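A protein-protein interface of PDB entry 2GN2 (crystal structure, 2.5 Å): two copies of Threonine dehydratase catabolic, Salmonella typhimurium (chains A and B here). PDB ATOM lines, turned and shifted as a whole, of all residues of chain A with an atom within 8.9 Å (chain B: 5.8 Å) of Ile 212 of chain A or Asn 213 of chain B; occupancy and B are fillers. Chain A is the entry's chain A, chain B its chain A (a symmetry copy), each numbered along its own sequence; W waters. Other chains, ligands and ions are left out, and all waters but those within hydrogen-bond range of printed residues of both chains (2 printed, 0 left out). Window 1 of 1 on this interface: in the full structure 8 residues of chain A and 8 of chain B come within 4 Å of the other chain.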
ATOM      1  N   ILE A  24       9.327  27.162  11.620  1.00  0.00           N
ATOM      2  CA  ILE A  24       8.436  27.796  10.640  1.00  0.00           C
ATOM      3  C   ILE A  24       7.227  28.483  11.281  1.00  0.00           C
ATOM      4  O   ILE A  24       6.815  29.548  10.832  1.00  0.00           O
ATOM      5  CB  ILE A  24       7.970  26.787   9.563  1.00  0.00           C
ATOM      6  CG1 ILE A  24       7.174  27.494   8.460  1.00  0.00           C
ATOM      7  CG2 ILE A  24       7.146  25.639  10.186  1.00  0.00           C
ATOM      8  CD1 ILE A  24       7.964  28.524   7.693  1.00  0.00           C
ATOM      9  N   GLU A  25       6.685  27.887  12.341  1.00  0.00           N
ATOM     10  CA  GLU A  25       5.573  28.484  13.082  1.00  0.00           C
ATOM     11  C   GLU A  25       5.924  29.853  13.675  1.00  0.00           C
ATOM     12  O   GLU A  25       5.079  30.741  13.722  1.00  0.00           O
ATOM     13  CB  GLU A  25       5.112  27.552  14.201  1.00  0.00           C
ATOM     14  CG  GLU A  25       4.499  26.235  13.716  1.00  0.00           C
ATOM     15  CD  GLU A  25       5.489  25.066  13.646  1.00  0.00           C
ATOM     16  OE1 GLU A  25       6.722  25.293  13.601  1.00  0.00           O
ATOM     17  OE2 GLU A  25       5.013  23.906  13.629  1.00  0.00           O
ATOM     18  N   ILE A  27       7.950  32.051  12.402  1.00  0.00           N
ATOM     19  CA  ILE A  27       7.904  32.988  11.279  1.00  0.00           C
ATOM     20  C   ILE A  27       6.454  33.359  10.954  1.00  0.00           C
ATOM     21  O   ILE A  27       6.157  34.517  10.650  1.00  0.00           O
ATOM     22  CB  ILE A  27       8.538  32.409   9.980  1.00  0.00           C
ATOM     23  CG1 ILE A  27       9.893  31.733  10.232  1.00  0.00           C
ATOM     24  CG2 ILE A  27       8.674  33.490   8.931  1.00  0.00           C
ATOM     25  CD1 ILE A  27      10.907  32.579  10.871  1.00  0.00           C
ATOM     26  N   LEU A  28       5.565  32.363  10.998  1.00  0.00           N
ATOM     27  CA  LEU A  28       4.136  32.578  10.725  1.00  0.00           C
ATOM     28  C   LEU A  28       3.496  33.503  11.760  1.00  0.00           C
ATOM     29  O   LEU A  28       2.678  34.354  11.413  1.00  0.00           O
ATOM     30  CB  LEU A  28       3.375  31.241  10.678  1.00  0.00           C
ATOM     31  CG  LEU A  28       3.779  30.259   9.570  1.00  0.00           C
ATOM     32  CD1 LEU A  28       3.081  28.934   9.752  1.00  0.00           C
ATOM     33  CD2 LEU A  28       3.503  30.842   8.183  1.00  0.00           C
ATOM     34  N   GLY A 176      12.911  36.442   9.078  1.00  0.00           N
ATOM     35  CA  GLY A 176      12.490  35.366   8.177  1.00  0.00           C
ATOM     36  C   GLY A 176      11.260  35.674   7.341  1.00  0.00           C
ATOM     37  O   GLY A 176      11.009  35.023   6.326  1.00  0.00           O
ATOM     38  N   GLY A 179      11.944  35.768   3.699  1.00  0.00           N
ATOM     39  CA  GLY A 179      11.910  34.531   2.935  1.00  0.00           C
ATOM     40  C   GLY A 179      10.520  34.189   2.422  1.00  0.00           C
ATOM     41  O   GLY A 179      10.373  33.713   1.287  1.00  0.00           O
ATOM     42  N   LEU A 180       9.494  34.418   3.241  1.00  0.00           N
ATOM     43  CA  LEU A 180       8.121  34.108   2.824  1.00  0.00           C
ATOM     44  C   LEU A 180       7.700  35.021   1.679  1.00  0.00           C
ATOM     45  O   LEU A 180       7.011  34.586   0.758  1.00  0.00           O
ATOM     46  CB  LEU A 180       7.120  34.276   3.967  1.00  0.00           C
ATOM     47  CG  LEU A 180       7.294  33.468   5.243  1.00  0.00           C
ATOM     48  CD1 LEU A 180       6.163  33.835   6.194  1.00  0.00           C
ATOM     49  CD2 LEU A 180       7.337  31.953   4.991  1.00  0.00           C
ATOM     50  N   GLU A 181       8.108  36.285   1.759  1.00  0.00           N
ATOM     51  CA  GLU A 181       7.839  37.268   0.706  1.00  0.00           C
ATOM     52  C   GLU A 181       8.510  36.891  -0.617  1.00  0.00           C
ATOM     53  O   GLU A 181       7.969  37.149  -1.693  1.00  0.00           O
ATOM     54  CB  GLU A 181       8.313  38.651   1.135  1.00  0.00           C
ATOM     55  CG  GLU A 181       7.507  39.263   2.266  1.00  0.00           C
ATOM     56  CD  GLU A 181       7.990  40.677   2.663  1.00  0.00           C
ATOM     57  OE1 GLU A 181       8.831  41.291   1.950  1.00  0.00           O
ATOM     58  OE2 GLU A 181       7.511  41.170   3.706  1.00  0.00           O
ATOM     59  N   MET A 183       9.291  33.735  -1.821  1.00  0.00           N
ATOM     60  CA  MET A 183       8.593  32.620  -2.447  1.00  0.00           C
ATOM     61  C   MET A 183       7.202  33.069  -2.917  1.00  0.00           C
ATOM     62  O   MET A 183       6.670  32.553  -3.896  1.00  0.00           O
ATOM     63  CB  MET A 183       8.506  31.454  -1.470  1.00  0.00           C
ATOM     64  CG  MET A 183       9.858  30.874  -1.132  1.00  0.00           C
ATOM     65  SD  MET A 183       9.804  29.612   0.140  1.00  0.00           S
ATOM     66  CE  MET A 183       9.388  30.560   1.589  1.00  0.00           C
ATOM     67  N   GLU A 184       6.632  34.043  -2.219  1.00  0.00           N
ATOM     68  CA  GLU A 184       5.397  34.705  -2.641  1.00  0.00           C
ATOM     69  C   GLU A 184       5.588  35.466  -3.971  1.00  0.00           C
ATOM     70  O   GLU A 184       4.772  35.343  -4.876  1.00  0.00           O
ATOM     71  CB  GLU A 184       4.932  35.668  -1.538  1.00  0.00           C
ATOM     72  CG  GLU A 184       3.477  36.074  -1.581  1.00  0.00           C
ATOM     73  CD  GLU A 184       3.050  36.780  -0.287  1.00  0.00           C
ATOM     74  OE1 GLU A 184       3.669  37.832   0.069  1.00  0.00           O
ATOM     75  OE2 GLU A 184       2.096  36.274   0.369  1.00  0.00           O
ATOM     76  N   TYR A 187       8.017  32.097  -7.007  1.00  0.00           N
ATOM     77  CA  TYR A 187       7.845  30.713  -6.561  1.00  0.00           C
ATOM     78  C   TYR A 187       8.963  29.785  -7.031  1.00  0.00           C
ATOM     79  O   TYR A 187       9.345  28.848  -6.328  1.00  0.00           O
ATOM     80  CB  TYR A 187       6.476  30.167  -7.008  1.00  0.00           C
ATOM     81  CG  TYR A 187       6.343  29.895  -8.494  1.00  0.00           C
ATOM     82  CD1 TYR A 187       5.851  30.864  -9.358  1.00  0.00           C
ATOM     83  CD2 TYR A 187       6.693  28.664  -9.027  1.00  0.00           C
ATOM     84  CE1 TYR A 187       5.719  30.625 -10.709  1.00  0.00           C
ATOM     85  CE2 TYR A 187       6.568  28.410 -10.383  1.00  0.00           C
ATOM     86  CZ  TYR A 187       6.079  29.398 -11.219  1.00  0.00           C
ATOM     87  OH  TYR A 187       5.950  29.150 -12.567  1.00  0.00           O
ATOM     88  N   ASP A 188       9.489  30.064  -8.220  1.00  0.00           N
ATOM     89  CA  ASP A 188      10.506  29.218  -8.855  1.00  0.00           C
ATOM     90  C   ASP A 188      11.911  29.764  -8.663  1.00  0.00           C
ATOM     91  O   ASP A 188      12.773  29.544  -9.509  1.00  0.00           O
ATOM     92  CB  ASP A 188      10.203  29.061 -10.354  1.00  0.00           C
ATOM     93  CG  ASP A 188      10.065  30.403 -11.076  1.00  0.00           C
ATOM     94  OD1 ASP A 188      10.217  30.426 -12.313  1.00  0.00           O
ATOM     95  OD2 ASP A 188       9.809  31.431 -10.408  1.00  0.00           O
ATOM     96  N   VAL A 189      12.136  30.489  -7.565  1.00  0.00           N
ATOM     97  CA  VAL A 189      13.481  30.946  -7.189  1.00  0.00           C
ATOM     98  C   VAL A 189      14.400  29.750  -6.890  1.00  0.00           C
ATOM     99  O   VAL A 189      13.963  28.748  -6.312  1.00  0.00           O
ATOM    100  CB  VAL A 189      13.437  31.885  -5.955  1.00  0.00           C
ATOM    101  CG1 VAL A 189      12.992  31.130  -4.701  1.00  0.00           C
ATOM    102  CG2 VAL A 189      14.804  32.545  -5.711  1.00  0.00           C
ATOM    103  N   ILE A 205      15.716  33.706   7.295  1.00  0.00           N
ATOM    104  CA  ILE A 205      15.406  33.376   5.911  1.00  0.00           C
ATOM    105  C   ILE A 205      15.565  31.874   5.649  1.00  0.00           C
ATOM    106  O   ILE A 205      14.661  31.249   5.089  1.00  0.00           O
ATOM    107  CB  ILE A 205      16.244  34.237   4.931  1.00  0.00           C
ATOM    108  CG1 ILE A 205      15.683  35.671   4.904  1.00  0.00           C
ATOM    109  CG2 ILE A 205      16.209  33.660   3.524  1.00  0.00           C
ATOM    110  CD1 ILE A 205      16.647  36.727   4.333  1.00  0.00           C
ATOM    111  N   ALA A 206      16.687  31.295   6.079  1.00  0.00           N
ATOM    112  CA  ALA A 206      16.935  29.856   5.890  1.00  0.00           C
ATOM    113  C   ALA A 206      15.782  29.004   6.403  1.00  0.00           C
ATOM    114  O   ALA A 206      15.294  28.125   5.695  1.00  0.00           O
ATOM    115  CB  ALA A 206      18.233  29.443   6.565  1.00  0.00           C
ATOM    116  N   ILE A 207      15.336  29.283   7.625  1.00  0.00           N
ATOM    117  CA  ILE A 207      14.211  28.563   8.215  1.00  0.00           C
ATOM    118  C   ILE A 207      12.949  28.709   7.367  1.00  0.00           C
ATOM    119  O   ILE A 207      12.249  27.718   7.127  1.00  0.00           O
ATOM    120  CB  ILE A 207      13.909  29.040   9.653  1.00  0.00           C
ATOM    121  CG1 ILE A 207      15.033  28.626  10.599  1.00  0.00           C
ATOM    122  CG2 ILE A 207      12.601  28.439  10.168  1.00  0.00           C
ATOM    123  CD1 ILE A 207      15.130  29.493  11.830  1.00  0.00           C
ATOM    124  N   ALA A 208      12.653  29.936   6.937  1.00  0.00           N
ATOM    125  CA  ALA A 208      11.488  30.179   6.089  1.00  0.00           C
ATOM    126  C   ALA A 208      11.630  29.433   4.772  1.00  0.00           C
ATOM    127  O   ALA A 208      10.732  28.695   4.374  1.00  0.00           O
ATOM    128  CB  ALA A 208      11.294  31.676   5.828  1.00  0.00           C
ATOM    129  N   ILE A 209      12.769  29.610   4.109  1.00  0.00           N
ATOM    130  CA  ILE A 209      12.992  28.989   2.805  1.00  0.00           C
ATOM    131  C   ILE A 209      13.036  27.456   2.901  1.00  0.00           C
ATOM    132  O   ILE A 209      12.266  26.771   2.226  1.00  0.00           O
ATOM    133  CB  ILE A 209      14.294  29.489   2.148  1.00  0.00           C
ATOM    134  CG1 ILE A 209      14.227  30.992   1.870  1.00  0.00           C
ATOM    135  CG2 ILE A 209      14.566  28.736   0.857  1.00  0.00           C
ATOM    136  CD1 ILE A 209      13.245  31.404   0.793  1.00  0.00           C
ATOM    137  N   LYS A 210      13.928  26.929   3.737  1.00  0.00           N
ATOM    138  CA  LYS A 210      14.126  25.474   3.826  1.00  0.00           C
ATOM    139  C   LYS A 210      12.910  24.703   4.361  1.00  0.00           C
ATOM    140  O   LYS A 210      12.735  23.525   4.033  1.00  0.00           O
ATOM    141  CB  LYS A 210      15.373  25.134   4.662  1.00  0.00           C
ATOM    142  CG  LYS A 210      16.686  25.717   4.122  1.00  0.00           C
ATOM    143  CD  LYS A 210      16.964  25.244   2.700  1.00  0.00           C
ATOM    144  CE  LYS A 210      18.404  25.495   2.284  1.00  0.00           C
ATOM    145  NZ  LYS A 210      18.713  24.900   0.947  1.00  0.00           N
ATOM    146  N   SER A 211      12.077  25.344   5.179  1.00  0.00           N
ATOM    147  CA  SER A 211      10.881  24.679   5.709  1.00  0.00           C
ATOM    148  C   SER A 211       9.834  24.431   4.634  1.00  0.00           C
ATOM    149  O   SER A 211       9.089  23.469   4.701  1.00  0.00           O
ATOM    150  CB  SER A 211      10.240  25.503   6.818  1.00  0.00           C
ATOM    151  OG  SER A 211      11.112  25.605   7.916  1.00  0.00           O
ATOM    152  N   ILE A 212       9.782  25.318   3.650  1.00  0.00           N
ATOM    153  CA  ILE A 212       8.764  25.268   2.623  1.00  0.00           C
ATOM    154  C   ILE A 212       9.295  24.586   1.372  1.00  0.00           C
ATOM    155  O   ILE A 212       8.627  23.726   0.793  1.00  0.00           O
ATOM    156  CB  ILE A 212       8.246  26.689   2.336  1.00  0.00           C
ATOM    157  CG1 ILE A 212       7.360  27.129   3.505  1.00  0.00           C
ATOM    158  CG2 ILE A 212       7.464  26.743   1.007  1.00  0.00           C
ATOM    159  CD1 ILE A 212       7.152  28.600   3.590  1.00  0.00           C
ATOM    160  N   ASN A 213      10.495  24.980   0.956  1.00  0.00           N
ATOM    161  CA  ASN A 213      11.140  24.386  -0.207  1.00  0.00           C
ATOM    162  C   ASN A 213      12.645  24.265   0.007  1.00  0.00           C
ATOM    163  O   ASN A 213      13.388  25.207  -0.245  1.00  0.00           O
ATOM    164  CB  ASN A 213      10.839  25.208  -1.458  1.00  0.00           C
ATOM    165  CG  ASN A 213      11.258  24.506  -2.724  1.00  0.00           C
ATOM    166  OD1 ASN A 213      11.857  23.435  -2.684  1.00  0.00           O
ATOM    167  ND2 ASN A 213      10.939  25.100  -3.862  1.00  0.00           N
ATOM    168  N   PRO A 214      13.100  23.090   0.461  1.00  0.00           N
ATOM    169  CA  PRO A 214      14.522  22.880   0.740  1.00  0.00           C
ATOM    170  C   PRO A 214      15.420  22.780  -0.496  1.00  0.00           C
ATOM    171  O   PRO A 214      16.637  22.775  -0.352  1.00  0.00           O
ATOM    172  CB  PRO A 214      14.534  21.564   1.519  1.00  0.00           C
ATOM    173  CG  PRO A 214      13.330  20.842   1.043  1.00  0.00           C
ATOM    174  CD  PRO A 214      12.300  21.883   0.740  1.00  0.00           C
ATOM    175  N   THR A 215      14.840  22.702  -1.690  1.00  0.00           N
ATOM    176  CA  THR A 215      15.637  22.710  -2.912  1.00  0.00           C
ATOM    177  C   THR A 215      16.149  24.115  -3.222  1.00  0.00           C
ATOM    178  O   THR A 215      17.024  24.279  -4.064  1.00  0.00           O
ATOM    179  CB  THR A 215      14.845  22.184  -4.135  1.00  0.00           C
ATOM    180  OG1 THR A 215      13.784  23.090  -4.457  1.00  0.00           O
ATOM    181  CG2 THR A 215      14.268  20.802  -3.859  1.00  0.00           C
ATOM    182  N   ILE A 216      15.605  25.131  -2.554  1.00  0.00           N
ATOM    183  CA  ILE A 216      16.084  26.490  -2.738  1.00  0.00           C
ATOM    184  C   ILE A 216      17.364  26.714  -1.938  1.00  0.00           C
ATOM    185  O   ILE A 216      17.380  26.569  -0.713  1.00  0.00           O
ATOM    186  CB  ILE A 216      15.061  27.544  -2.285  1.00  0.00           C
ATOM    187  CG1 ILE A 216      13.740  27.379  -3.040  1.00  0.00           C
ATOM    188  CG2 ILE A 216      15.648  28.952  -2.484  1.00  0.00           C
ATOM    189  CD1 ILE A 216      12.615  28.217  -2.505  1.00  0.00           C
ATOM    190  N   MET B 183       1.481  27.052  -7.475  1.00  0.00           N
ATOM    191  CA  MET B 183       2.596  27.524  -6.666  1.00  0.00           C
ATOM    192  C   MET B 183       2.705  29.053  -6.760  1.00  0.00           C
ATOM    193  O   MET B 183       3.143  29.714  -5.823  1.00  0.00           O
ATOM    194  CB  MET B 183       3.882  26.841  -7.114  1.00  0.00           C
ATOM    195  CG  MET B 183       3.872  25.353  -6.861  1.00  0.00           C
ATOM    196  SD  MET B 183       5.299  24.498  -7.527  1.00  0.00           S
ATOM    197  CE  MET B 183       5.022  24.619  -9.282  1.00  0.00           C
ATOM    198  N   TYR B 187       2.176  29.584  -2.544  1.00  0.00           N
ATOM    199  CA  TYR B 187       3.556  29.104  -2.459  1.00  0.00           C
ATOM    200  C   TYR B 187       3.750  28.011  -1.410  1.00  0.00           C
ATOM    201  O   TYR B 187       4.564  27.103  -1.585  1.00  0.00           O
ATOM    202  CB  TYR B 187       4.519  30.275  -2.189  1.00  0.00           C
ATOM    203  CG  TYR B 187       4.447  30.866  -0.795  1.00  0.00           C
ATOM    204  CD1 TYR B 187       3.613  31.941  -0.515  1.00  0.00           C
ATOM    205  CD2 TYR B 187       5.224  30.359   0.235  1.00  0.00           C
ATOM    206  CE1 TYR B 187       3.544  32.490   0.747  1.00  0.00           C
ATOM    207  CE2 TYR B 187       5.164  30.899   1.509  1.00  0.00           C
ATOM    208  CZ  TYR B 187       4.318  31.966   1.757  1.00  0.00           C
ATOM    209  OH  TYR B 187       4.257  32.508   3.021  1.00  0.00           O
ATOM    210  N   ASP B 188       2.984  28.101  -0.327  1.00  0.00           N
ATOM    211  CA  ASP B 188       3.110  27.185   0.812  1.00  0.00           C
ATOM    212  C   ASP B 188       2.068  26.079   0.780  1.00  0.00           C
ATOM    213  O   ASP B 188       1.670  25.584   1.831  1.00  0.00           O
ATOM    214  CB  ASP B 188       3.009  27.965   2.133  1.00  0.00           C
ATOM    215  CG  ASP B 188       1.733  28.803   2.232  1.00  0.00           C
ATOM    216  OD1 ASP B 188       1.341  29.150   3.362  1.00  0.00           O
ATOM    217  OD2 ASP B 188       1.123  29.110   1.182  1.00  0.00           O
ATOM    218  N   VAL B 189       1.614  25.707  -0.418  1.00  0.00           N
ATOM    219  CA  VAL B 189       0.721  24.554  -0.596  1.00  0.00           C
ATOM    220  C   VAL B 189       1.423  23.250  -0.180  1.00  0.00           C
ATOM    221  O   VAL B 189       2.623  23.076  -0.422  1.00  0.00           O
ATOM    222  CB  VAL B 189       0.234  24.433  -2.063  1.00  0.00           C
ATOM    223  CG1 VAL B 189       1.391  24.091  -3.004  1.00  0.00           C
ATOM    224  CG2 VAL B 189      -0.878  23.379  -2.195  1.00  0.00           C
ATOM    225  N   ALA B 208       5.445  19.558 -13.005  1.00  0.00           N
ATOM    226  CA  ALA B 208       5.537  20.968 -12.629  1.00  0.00           C
ATOM    227  C   ALA B 208       5.794  21.099 -11.137  1.00  0.00           C
ATOM    228  O   ALA B 208       6.728  21.782 -10.723  1.00  0.00           O
ATOM    229  CB  ALA B 208       4.265  21.730 -13.014  1.00  0.00           C
ATOM    230  N   ILE B 209       4.976  20.427 -10.332  1.00  0.00           N
ATOM    231  CA  ILE B 209       5.092  20.525  -8.878  1.00  0.00           C
ATOM    232  C   ILE B 209       6.420  19.943  -8.369  1.00  0.00           C
ATOM    233  O   ILE B 209       7.184  20.638  -7.697  1.00  0.00           O
ATOM    234  CB  ILE B 209       3.927  19.816  -8.162  1.00  0.00           C
ATOM    235  CG1 ILE B 209       2.589  20.478  -8.503  1.00  0.00           C
ATOM    236  CG2 ILE B 209       4.138  19.824  -6.657  1.00  0.00           C
ATOM    237  CD1 ILE B 209       2.399  21.872  -7.942  1.00  0.00           C
ATOM    238  N   LYS B 210       6.689  18.680  -8.694  1.00  0.00           N
ATOM    239  CA  LYS B 210       7.881  17.993  -8.171  1.00  0.00           C
ATOM    240  C   LYS B 210       9.213  18.584  -8.654  1.00  0.00           C
ATOM    241  O   LYS B 210      10.227  18.470  -7.956  1.00  0.00           O
ATOM    242  CB  LYS B 210       7.832  16.486  -8.479  1.00  0.00           C
ATOM    243  CG  LYS B 210       6.618  15.751  -7.895  1.00  0.00           C
ATOM    244  CD  LYS B 210       6.553  15.895  -6.379  1.00  0.00           C
ATOM    245  CE  LYS B 210       5.600  14.893  -5.748  1.00  0.00           C
ATOM    246  NZ  LYS B 210       5.648  14.938  -4.254  1.00  0.00           N
ATOM    247  N   SER B 211       9.228  19.204  -9.833  1.00  0.00           N
ATOM    248  CA  SER B 211      10.459  19.815 -10.347  1.00  0.00           C
ATOM    249  C   SER B 211      10.869  21.046  -9.553  1.00  0.00           C
ATOM    250  O   SER B 211      12.044  21.346  -9.431  1.00  0.00           O
ATOM    251  CB  SER B 211      10.304  20.220 -11.808  1.00  0.00           C
ATOM    252  OG  SER B 211      10.103  19.082 -12.610  1.00  0.00           O
ATOM    253  N   ILE B 212       9.883  21.760  -9.026  1.00  0.00           N
ATOM    254  CA  ILE B 212      10.120  23.012  -8.344  1.00  0.00           C
ATOM    255  C   ILE B 212      10.167  22.805  -6.838  1.00  0.00           C
ATOM    256  O   ILE B 212      11.060  23.317  -6.160  1.00  0.00           O
ATOM    257  CB  ILE B 212       9.050  24.040  -8.757  1.00  0.00           C
ATOM    258  CG1 ILE B 212       9.349  24.506 -10.184  1.00  0.00           C
ATOM    259  CG2 ILE B 212       9.020  25.239  -7.786  1.00  0.00           C
ATOM    260  CD1 ILE B 212       8.191  25.139 -10.872  1.00  0.00           C
ATOM    261  N   ASN B 213       9.197  22.057  -6.321  1.00  0.00           N
ATOM    262  CA  ASN B 213       9.139  21.747  -4.899  1.00  0.00           C
ATOM    263  C   ASN B 213       8.633  20.326  -4.673  1.00  0.00           C
ATOM    264  O   ASN B 213       7.431  20.092  -4.623  1.00  0.00           O
ATOM    265  CB  ASN B 213       8.252  22.754  -4.172  1.00  0.00           C
ATOM    266  CG  ASN B 213       8.361  22.642  -2.673  1.00  0.00           C
ATOM    267  OD1 ASN B 213       9.032  21.754  -2.154  1.00  0.00           O
ATOM    268  ND2 ASN B 213       7.708  23.547  -1.964  1.00  0.00           N
ATOM    269  N   PRO B 214       9.560  19.370  -4.518  1.00  0.00           N
ATOM    270  CA  PRO B 214       9.185  17.966  -4.336  1.00  0.00           C
ATOM    271  C   PRO B 214       8.571  17.629  -2.975  1.00  0.00           C
ATOM    272  O   PRO B 214       8.075  16.521  -2.800  1.00  0.00           O
ATOM    273  CB  PRO B 214      10.508  17.225  -4.526  1.00  0.00           C
ATOM    274  CG  PRO B 214      11.544  18.205  -4.124  1.00  0.00           C
ATOM    275  CD  PRO B 214      11.023  19.556  -4.505  1.00  0.00           C
ATOM    276  N   THR B 215       8.599  18.558  -2.023  1.00  0.00           N
ATOM    277  CA  THR B 215       7.939  18.337  -0.740  1.00  0.00           C
ATOM    278  C   THR B 215       6.424  18.479  -0.873  1.00  0.00           C
ATOM    279  O   THR B 215       5.691  18.098   0.031  1.00  0.00           O
ATOM    280  CB  THR B 215       8.440  19.312   0.354  1.00  0.00           C
ATOM    281  OG1 THR B 215       8.045  20.651   0.035  1.00  0.00           O
ATOM    282  CG2 THR B 215       9.955  19.248   0.491  1.00  0.00           C
ATOM    283  N   ILE B 216       5.951  19.031  -1.989  1.00  0.00           N
ATOM    284  CA  ILE B 216       4.522  19.137  -2.225  1.00  0.00           C
ATOM    285  C   ILE B 216       3.963  17.802  -2.706  1.00  0.00           C
ATOM    286  O   ILE B 216       4.384  17.273  -3.739  1.00  0.00           O
ATOM    287  CB  ILE B 216       4.174  20.196  -3.282  1.00  0.00           C
ATOM    288  CG1 ILE B 216       4.711  21.570  -2.872  1.00  0.00           C
ATOM    289  CG2 ILE B 216       2.651  20.232  -3.495  1.00  0.00           C
ATOM    290  CD1 ILE B 216       4.614  22.615  -3.945  1.00  0.00           C
HETATM  291  O   HOH W   1      13.219  24.739  -6.664  1.00  0.00           O
HETATM  292  O   HOH W   2       6.325  22.525   1.234  1.00  0.00           O
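Water W2 bridges O of Ile 212 of chain A (2.6 Å) and OG1 of Thr 215 of chain B (2.8 Å).
Water W1 bridges O of Ile 212 of chain B (2.6 Å) and OG1 of Thr 215 of chain A (2.8 Å).
Ile 212 of chain A touches three residues of chain B.
Asn 213 of chain B touches just these residues of chain A: Ile 212 (2.9 Å) and Asn 213 (3.3 Å).
Printed residues of chain A within 4 Å of Pro 214 of chain B: Thr 215.
Of the printed residues of chain B, Glu 184 of chain A touches Tyr 187.
Of the printed residues of chain B, Asn 213 of chain A touches Ile 212 and Asn 213.
Of the printed residues of chain A, Thr 215 of chain B touches Ile 212 and Pro 214.
Of the printed residues of chain A, Tyr 187 of chain B touches Leu 180 (3.5 Å), Met 183 (3.6 Å), Glu 184 (3.9 Å) and Ile 212 (3.7 Å).
Printed residues of chain B within 4 Å of Thr 215 of chain A: Ile 212 (3.2 Å) and Pro 214 (3.5 Å).
The nearest printed residue of chain B that does not touch Thr 215 of chain A is Asn 213 of chain B (4.9 Å).
Tyr 187 of chain A touches Ile 212 of chain B, and with the chains exchanged Ile 212 of chain A touches Tyr 187 of chain B.
Ile 212 of chain A touches Thr 215 of chain B, and with the chains exchanged Thr 215 of chain A touches Ile 212 of chain B.
Asn 213 of chain B touches its own counterpart, Asn 213 of chain A.
Pro 214 of chain A touches Thr 215 of chain B, and with the chains exchanged Thr 215 of chain A touches Pro 214 of chain B.
13 positions are printed for both chains.
The backbone carbonyl oxygen of Ile 212 of chain B lies within hydrogen-bond range of the side-chain amide nitrogen of Asn 213 of chain A (2.9 Å).
The backbone carbonyl oxygen of Ile 212 of chain A is in hydrogen-bond range of the side-chain hydroxyl of Thr 215 of chain B (3.2 Å).
The side-chain amide oxygen of Asn 213 of chain B sits close to the side-chain amide oxygen of Asn 213 of chain A (3.3 Å).
ND2 of Asn 213 of chain B lies within hydrogen-bond range of O of Ile 212 of chain A (2.9 Å).
O of Ile 212 of chain B lies within hydrogen-bond range of OG1 of Thr 215 of chain A, 3.2 Å away.
Of the 25 printed residues of chain A, 8 touch a printed residue of chain B.
Printed residues of chain A that touch a printed residue of chain B: Leu 180, Met 183, Glu 184, Tyr 187, Ile 212, Asn 213, Pro 214 and Thr 215.
Hydrophobic or aromatic side chains of chain A within 4 Å of the printed part of chain B: Leu 180, Met 183, Tyr 187, Ile 212 and Pro 214.
Along chain A the printed residues that touch a printed residue of chain B span positions 180 to 215.
Among the printed residues, 13 pairs touch across the chains.
Among the printed residues, pairs that only touch across the chains: Leu 180 of chain A with Tyr 187 of chain B (3.5 Å), Thr 215 of chain A with Pro 214 of chain B (3.5 Å), Pro 214 of chain A with Thr 215 of chain B (3.5 Å), Tyr 187 of chain A with Met 183 of chain B (3.6 Å), Met 183 of chain A with Tyr 187 of chain B (3.6 Å), Ile 212 of chain A with Tyr 187 of chain B (3.7 Å), Tyr 187 of chain A with Ile 212 of chain B (3.7 Å) and Glu 184 of chain A with Tyr 187 of chain B (3.9 Å).
The side-chain amide oxygen (OD1) of Asn 213 of chain B sits at hydrogen-bond distance from the side-chain hydroxyl (OG1) of Thr 215 of chain B (2.6 Å).
The side-chain amino group (NZ) of Lys 210 of chain A is in hydrogen-bond range of the backbone carbonyl oxygen (O) of Pro 214 of chain A.
The side-chain amide oxygen (OD1) of Asn 213 of chain A sits at hydrogen-bond distance from the side-chain hydroxyl (OG1) of Thr 215 of chain A.
The backbone carbonyl oxygen (O) of Pro 214 of chain B lies within hydrogen-bond range of the side-chain amino group (NZ) of Lys 210 of chain B (3.2 Å).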
